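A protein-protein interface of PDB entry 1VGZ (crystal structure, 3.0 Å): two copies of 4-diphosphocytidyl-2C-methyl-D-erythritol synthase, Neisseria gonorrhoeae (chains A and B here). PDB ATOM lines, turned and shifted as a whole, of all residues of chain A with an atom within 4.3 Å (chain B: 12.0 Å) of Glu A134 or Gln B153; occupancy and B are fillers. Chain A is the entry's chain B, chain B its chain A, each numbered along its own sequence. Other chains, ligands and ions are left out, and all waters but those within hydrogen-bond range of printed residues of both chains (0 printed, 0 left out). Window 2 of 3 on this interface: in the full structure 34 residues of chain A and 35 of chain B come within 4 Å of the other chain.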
ATOM      1  N   ALA A 132     -33.075   0.183   0.425  1.00  0.00           N
ATOM      2  CA  ALA A 132     -32.483   0.881   1.574  1.00  0.00           C
ATOM      3  C   ALA A 132     -32.180   2.275   1.039  1.00  0.00           C
ATOM      4  O   ALA A 132     -31.400   2.388   0.088  1.00  0.00           O
ATOM      5  CB  ALA A 132     -31.249   0.159   2.040  1.00  0.00           C
ATOM      6  N   ALA A 133     -32.811   3.310   1.564  1.00  0.00           N
ATOM      7  CA  ALA A 133     -32.631   4.653   1.045  1.00  0.00           C
ATOM      8  C   ALA A 133     -31.189   5.067   0.872  1.00  0.00           C
ATOM      9  O   ALA A 133     -30.785   5.539  -0.191  1.00  0.00           O
ATOM     10  CB  ALA A 133     -33.360   5.671   1.901  1.00  0.00           C
ATOM     11  N   GLU A 134     -30.379   4.854   1.886  1.00  0.00           N
ATOM     12  CA  GLU A 134     -28.979   5.202   1.972  1.00  0.00           C
ATOM     13  C   GLU A 134     -28.107   4.661   0.853  1.00  0.00           C
ATOM     14  O   GLU A 134     -27.109   5.291   0.468  1.00  0.00           O
ATOM     15  CB  GLU A 134     -28.428   4.751   3.337  1.00  0.00           C
ATOM     16  CG  GLU A 134     -28.689   3.292   3.639  1.00  0.00           C
ATOM     17  CD  GLU A 134     -29.847   3.053   4.582  1.00  0.00           C
ATOM     18  OE1 GLU A 134     -30.792   3.871   4.617  1.00  0.00           O
ATOM     19  OE2 GLU A 134     -29.824   2.024   5.303  1.00  0.00           O
ATOM     20  N   GLY A 135     -28.489   3.527   0.281  1.00  0.00           N
ATOM     21  CA  GLY A 135     -27.714   2.956  -0.811  1.00  0.00           C
ATOM     22  C   GLY A 135     -26.817   1.860  -0.239  1.00  0.00           C
ATOM     23  O   GLY A 135     -26.927   1.501   0.936  1.00  0.00           O
ATOM     24  N   PHE A 172     -27.275   3.512  -5.687  1.00  0.00           N
ATOM     25  CA  PHE A 172     -27.906   4.643  -5.050  1.00  0.00           C
ATOM     26  C   PHE A 172     -29.135   5.136  -5.819  1.00  0.00           C
ATOM     27  O   PHE A 172     -29.148   5.013  -7.048  1.00  0.00           O
ATOM     28  CB  PHE A 172     -26.912   5.835  -5.033  1.00  0.00           C
ATOM     29  CG  PHE A 172     -25.752   5.635  -4.113  1.00  0.00           C
ATOM     30  CD1 PHE A 172     -24.456   5.617  -4.603  1.00  0.00           C
ATOM     31  CD2 PHE A 172     -25.946   5.372  -2.766  1.00  0.00           C
ATOM     32  CE1 PHE A 172     -23.375   5.391  -3.770  1.00  0.00           C
ATOM     33  CE2 PHE A 172     -24.877   5.152  -1.920  1.00  0.00           C
ATOM     34  CZ  PHE A 172     -23.601   5.156  -2.427  1.00  0.00           C
ATOM     35  N   LEU A 176     -30.763  11.083  -5.312  1.00  0.00           N
ATOM     36  CA  LEU A 176     -29.740  11.201  -4.268  1.00  0.00           C
ATOM     37  C   LEU A 176     -28.366  11.355  -4.915  1.00  0.00           C
ATOM     38  O   LEU A 176     -27.715  12.374  -4.735  1.00  0.00           O
ATOM     39  CB  LEU A 176     -29.749   9.981  -3.367  1.00  0.00           C
ATOM     40  CG  LEU A 176     -28.684   9.903  -2.273  1.00  0.00           C
ATOM     41  CD1 LEU A 176     -28.745  11.113  -1.361  1.00  0.00           C
ATOM     42  CD2 LEU A 176     -28.844   8.612  -1.474  1.00  0.00           C
ATOM     43  N   VAL A 196     -21.843  10.458  -1.595  1.00  0.00           N
ATOM     44  CA  VAL A 196     -23.048  10.289  -0.787  1.00  0.00           C
ATOM     45  C   VAL A 196     -22.796  10.412   0.701  1.00  0.00           C
ATOM     46  O   VAL A 196     -23.649  10.930   1.447  1.00  0.00           O
ATOM     47  CB  VAL A 196     -23.739   8.955  -1.140  1.00  0.00           C
ATOM     48  CG1 VAL A 196     -24.684   8.474  -0.057  1.00  0.00           C
ATOM     49  CG2 VAL A 196     -24.525   9.091  -2.449  1.00  0.00           C
ATOM     50  N   VAL A 201     -25.238  10.840   4.433  1.00  0.00           N
ATOM     51  CA  VAL A 201     -25.838   9.524   4.211  1.00  0.00           C
ATOM     52  C   VAL A 201     -24.776   8.437   4.225  1.00  0.00           C
ATOM     53  O   VAL A 201     -23.830   8.459   3.442  1.00  0.00           O
ATOM     54  CB  VAL A 201     -26.664   9.493   2.905  1.00  0.00           C
ATOM     55  CG1 VAL A 201     -26.968   8.080   2.454  1.00  0.00           C
ATOM     56  CG2 VAL A 201     -27.969  10.252   3.084  1.00  0.00           C
ATOM     57  N   ARG A 202     -24.927   7.450   5.079  1.00  0.00           N
ATOM     58  CA  ARG A 202     -24.042   6.327   5.234  1.00  0.00           C
ATOM     59  C   ARG A 202     -24.536   5.118   4.444  1.00  0.00           C
ATOM     60  O   ARG A 202     -25.348   4.359   5.001  1.00  0.00           O
ATOM     61  CB  ARG A 202     -24.086   5.882   6.714  1.00  0.00           C
ATOM     62  CG  ARG A 202     -23.644   6.941   7.704  1.00  0.00           C
ATOM     63  CD  ARG A 202     -23.597   6.329   9.101  1.00  0.00           C
ATOM     64  NE  ARG A 202     -22.593   6.981   9.929  1.00  0.00           N
ATOM     65  CZ  ARG A 202     -21.989   6.407  10.967  1.00  0.00           C
ATOM     66  NH1 ARG A 202     -22.271   5.157  11.326  1.00  0.00           N
ATOM     67  NH2 ARG A 202     -21.091   7.104  11.651  1.00  0.00           N
ATOM     68  N   PRO A 203     -24.009   4.894   3.253  1.00  0.00           N
ATOM     69  CA  PRO A 203     -24.433   3.766   2.431  1.00  0.00           C
ATOM     70  C   PRO A 203     -24.068   2.463   3.105  1.00  0.00           C
ATOM     71  O   PRO A 203     -23.141   2.496   3.916  1.00  0.00           O
ATOM     72  CB  PRO A 203     -23.683   3.945   1.139  1.00  0.00           C
ATOM     73  CG  PRO A 203     -23.026   5.270   1.167  1.00  0.00           C
ATOM     74  CD  PRO A 203     -22.985   5.721   2.594  1.00  0.00           C
ATOM     75  N   LEU A 204     -24.735   1.357   2.828  1.00  0.00           N
ATOM     76  CA  LEU A 204     -24.393   0.086   3.459  1.00  0.00           C
ATOM     77  C   LEU A 204     -23.104  -0.504   2.851  1.00  0.00           C
ATOM     78  O   LEU A 204     -22.573  -0.021   1.847  1.00  0.00           O
ATOM     79  CB  LEU A 204     -25.505  -0.930   3.274  1.00  0.00           C
ATOM     80  CG  LEU A 204     -26.968  -0.664   3.519  1.00  0.00           C
ATOM     81  CD1 LEU A 204     -27.701  -1.940   3.972  1.00  0.00           C
ATOM     82  CD2 LEU A 204     -27.233   0.426   4.548  1.00  0.00           C
ATOM     83  N   LEU B 146     -10.858   2.892   0.077  1.00  0.00           N
ATOM     84  CA  LEU B 146     -10.988   2.221   1.375  1.00  0.00           C
ATOM     85  C   LEU B 146     -12.100   2.872   2.195  1.00  0.00           C
ATOM     86  O   LEU B 146     -12.170   4.102   2.237  1.00  0.00           O
ATOM     87  CB  LEU B 146      -9.704   2.323   2.192  1.00  0.00           C
ATOM     88  CG  LEU B 146      -8.492   1.459   1.926  1.00  0.00           C
ATOM     89  CD1 LEU B 146      -7.659   1.404   3.214  1.00  0.00           C
ATOM     90  CD2 LEU B 146      -8.816   0.051   1.467  1.00  0.00           C
ATOM     91  N   LYS B 147     -12.896   2.076   2.893  1.00  0.00           N
ATOM     92  CA  LYS B 147     -13.975   2.625   3.684  1.00  0.00           C
ATOM     93  C   LYS B 147     -13.961   2.112   5.116  1.00  0.00           C
ATOM     94  O   LYS B 147     -13.868   0.912   5.348  1.00  0.00           O
ATOM     95  CB  LYS B 147     -15.349   2.239   3.092  1.00  0.00           C
ATOM     96  CG  LYS B 147     -15.587   2.552   1.644  1.00  0.00           C
ATOM     97  CD  LYS B 147     -15.839   4.030   1.370  1.00  0.00           C
ATOM     98  CE  LYS B 147     -16.120   4.239  -0.114  1.00  0.00           C
ATOM     99  NZ  LYS B 147     -16.141   5.668  -0.510  1.00  0.00           N
ATOM    100  N   ARG B 148     -14.200   3.015   6.052  1.00  0.00           N
ATOM    101  CA  ARG B 148     -14.275   2.651   7.463  1.00  0.00           C
ATOM    102  C   ARG B 148     -15.720   2.268   7.790  1.00  0.00           C
ATOM    103  O   ARG B 148     -16.638   3.088   7.726  1.00  0.00           O
ATOM    104  CB  ARG B 148     -13.813   3.798   8.355  1.00  0.00           C
ATOM    105  N   ALA B 149     -15.926   0.997   8.100  1.00  0.00           N
ATOM    106  CA  ALA B 149     -17.259   0.514   8.444  1.00  0.00           C
ATOM    107  C   ALA B 149     -17.531   0.919   9.896  1.00  0.00           C
ATOM    108  O   ALA B 149     -16.646   1.484  10.537  1.00  0.00           O
ATOM    109  CB  ALA B 149     -17.348  -0.991   8.328  1.00  0.00           C
ATOM    110  N   GLU B 150     -18.790   0.870  10.304  1.00  0.00           N
ATOM    111  CA  GLU B 150     -19.185   1.208  11.663  1.00  0.00           C
ATOM    112  C   GLU B 150     -20.081   0.098  12.209  1.00  0.00           C
ATOM    113  O   GLU B 150     -19.813  -0.388  13.318  1.00  0.00           O
ATOM    114  CB  GLU B 150     -19.833   2.564  11.819  1.00  0.00           C
ATOM    115  CG  GLU B 150     -19.656   3.149  13.221  1.00  0.00           C
ATOM    116  CD  GLU B 150     -18.663   4.289  13.275  1.00  0.00           C
ATOM    117  OE1 GLU B 150     -19.082   5.462  13.435  1.00  0.00           O
ATOM    118  OE2 GLU B 150     -17.441   4.032  13.144  1.00  0.00           O
ATOM    119  N   SER B 151     -21.086  -0.339  11.459  1.00  0.00           N
ATOM    120  CA  SER B 151     -21.910  -1.445  11.987  1.00  0.00           C
ATOM    121  C   SER B 151     -22.766  -2.015  10.864  1.00  0.00           C
ATOM    122  O   SER B 151     -23.905  -2.449  11.042  1.00  0.00           O
ATOM    123  CB  SER B 151     -22.736  -0.956  13.163  1.00  0.00           C
ATOM    124  OG  SER B 151     -22.965  -1.981  14.119  1.00  0.00           O
ATOM    125  N   GLY B 152     -22.176  -2.030   9.675  1.00  0.00           N
ATOM    126  CA  GLY B 152     -22.817  -2.500   8.453  1.00  0.00           C
ATOM    127  C   GLY B 152     -22.885  -1.312   7.482  1.00  0.00           C
ATOM    128  O   GLY B 152     -23.277  -1.448   6.328  1.00  0.00           O
ATOM    129  N   GLN B 153     -22.476  -0.141   7.979  1.00  0.00           N
ATOM    130  CA  GLN B 153     -22.488   1.075   7.210  1.00  0.00           C
ATOM    131  C   GLN B 153     -21.146   1.816   7.185  1.00  0.00           C
ATOM    132  O   GLN B 153     -20.325   1.771   8.093  1.00  0.00           O
ATOM    133  CB  GLN B 153     -23.531   2.070   7.753  1.00  0.00           C
ATOM    134  CG  GLN B 153     -24.973   1.633   7.687  1.00  0.00           C
ATOM    135  CD  GLN B 153     -25.962   2.752   7.422  1.00  0.00           C
ATOM    136  OE1 GLN B 153     -26.692   2.739   6.425  1.00  0.00           O
ATOM    137  NE2 GLN B 153     -25.978   3.757   8.292  1.00  0.00           N
ATOM    138  N   ILE B 154     -21.010   2.638   6.141  1.00  0.00           N
ATOM    139  CA  ILE B 154     -19.845   3.453   5.919  1.00  0.00           C
ATOM    140  C   ILE B 154     -19.827   4.680   6.824  1.00  0.00           C
ATOM    141  O   ILE B 154     -20.533   5.668   6.648  1.00  0.00           O
ATOM    142  CB  ILE B 154     -19.744   3.871   4.441  1.00  0.00           C
ATOM    143  CG1 ILE B 154     -19.564   2.634   3.556  1.00  0.00           C
ATOM    144  CG2 ILE B 154     -18.616   4.870   4.255  1.00  0.00           C
ATOM    145  CD1 ILE B 154     -19.283   2.937   2.089  1.00  0.00           C
ATOM    146  N   SER B 155     -18.929   4.627   7.819  1.00  0.00           N
ATOM    147  CA  SER B 155     -18.737   5.738   8.740  1.00  0.00           C
ATOM    148  C   SER B 155     -17.638   6.667   8.249  1.00  0.00           C
ATOM    149  O   SER B 155     -17.533   7.785   8.755  1.00  0.00           O
ATOM    150  CB  SER B 155     -18.457   5.266  10.148  1.00  0.00           C
ATOM    151  OG  SER B 155     -17.481   4.251  10.178  1.00  0.00           O
ATOM    152  N   ALA B 156     -16.828   6.236   7.284  1.00  0.00           N
ATOM    153  CA  ALA B 156     -15.810   7.141   6.747  1.00  0.00           C
ATOM    154  C   ALA B 156     -14.975   6.531   5.637  1.00  0.00           C
ATOM    155  O   ALA B 156     -14.793   5.326   5.591  1.00  0.00           O
ATOM    156  CB  ALA B 156     -14.899   7.650   7.858  1.00  0.00           C
ATOM    157  N   THR B 157     -14.509   7.365   4.722  1.00  0.00           N
ATOM    158  CA  THR B 157     -13.643   6.934   3.632  1.00  0.00           C
ATOM    159  C   THR B 157     -12.208   7.322   4.049  1.00  0.00           C
ATOM    160  O   THR B 157     -12.029   8.444   4.539  1.00  0.00           O
ATOM    161  CB  THR B 157     -13.937   7.597   2.284  1.00  0.00           C
ATOM    162  OG1 THR B 157     -12.865   7.326   1.354  1.00  0.00           O
ATOM    163  CG2 THR B 157     -14.017   9.115   2.419  1.00  0.00           C
ATOM    164  N   VAL B 158     -11.277   6.378   3.982  1.00  0.00           N
ATOM    165  CA  VAL B 158      -9.897   6.671   4.364  1.00  0.00           C
ATOM    166  C   VAL B 158      -9.032   6.843   3.125  1.00  0.00           C
ATOM    167  O   VAL B 158      -9.183   6.166   2.109  1.00  0.00           O
ATOM    168  CB  VAL B 158      -9.316   5.645   5.334  1.00  0.00           C
ATOM    169  CG1 VAL B 158     -10.348   5.249   6.384  1.00  0.00           C
ATOM    170  CG2 VAL B 158      -8.780   4.404   4.641  1.00  0.00           C
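The side-chain carboxylate (OE1) of Glu B150 lies within salt-bridge range of the guanidinium group (NH2) of Arg A202 (3.1 Å). OE1 of Gln B153 lies close to OE2 of Glu A134, at 3.4 Å. The side-chain amide oxygen (OE1) of Gln B153 lies close to the backbone carbonyl oxygen (O) of Arg A202 (2.5 Å). O of Pro A203 sits at hydrogen-bond distance from N of Ile B154 (3.1 Å).
O of Arg B148 sits at hydrogen-bond distance from N of Ser B155, at 2.8 Å. O of Ala B149 is in hydrogen-bond range of OG of Ser B155 (2.9 Å). The side-chain carboxylate (OE2) of Glu B150 lies within hydrogen-bond range of the side-chain hydroxyl (OG) of Ser B155 (3.0 Å). O of Gly A135 is in hydrogen-bond range of N of Leu A204 (2.9 Å).
CG of Arg A202 touches O of Ile B154, at 3.5 Å. NH2 of Arg A202 touches CB of Ser B155, at 3.5 Å. O of Pro A203 touches CA of Gln B153, at 3.6 Å. Gly B152 touches Leu A204 (O to CA, 3.4 Å). Gln B153 touches Leu A204 (OE1 to CD2, 3.0 Å).
Of chain B, only Gln B153 comes within 4 Å of Glu A134. Gln B153 touches just these residues of chain A: Glu A134, Arg A202, Pro A203 and Leu A204. Ala A132 touches none of the printed residues of chain B. No residue of chain B comes within 4 Å of Ala A133. No residue of chain B comes within 4 Å of Gly A135. No residue of chain B comes within 4 Å of Phe A172. No residue of chain B comes within 4 Å of Val A196. No residue of chain B comes within 4 Å of Val A201. Of chain B, only Glu B150, Gln B153, Ile B154 and Ser B155 come within 4 Å of Arg A202. Pro A203 touches two residues of chain B. Leu A204 touches just these residues of chain B: Gly B152 (3.4 Å) and Gln B153 (3.0 Å). Of the printed residues of chain A, Glu B150 touches Arg A202. Printed residues of chain A within 4 Å of Ile B154: Arg A202 (3.5 Å) and Pro A203 (3.1 Å). Of the printed residues of chain A, Gly B152 touches Leu A204. Ala B156 touches none of the printed residues of chain A. Val B158 touches none of the printed residues of chain A. The nearest residue of chain B that does not touch Glu A134 is Gly B152 (7.5 Å). The nearest printed residue of chain A that does not touch Gln B153 is Gly A135 (5.6 Å).
Printed residues of chain B that touch a printed residue of chain A: Glu B150, Gly B152, Gln B153, Ile B154 and Ser B155. Hydrophobic or aromatic side chains of chain B that line the printed part of chain A: Ile B154. Among the printed residues, Asp or Glu carboxylates within 4 Å of a Lys or Arg side-chain nitrogen of the other chain: Arg A202 with Glu B150 (3.1 Å).
No position is printed for both chains. Of the 9 pairs that touch across the chains among the printed residues, none has its exchanged pair printed and touching as well.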
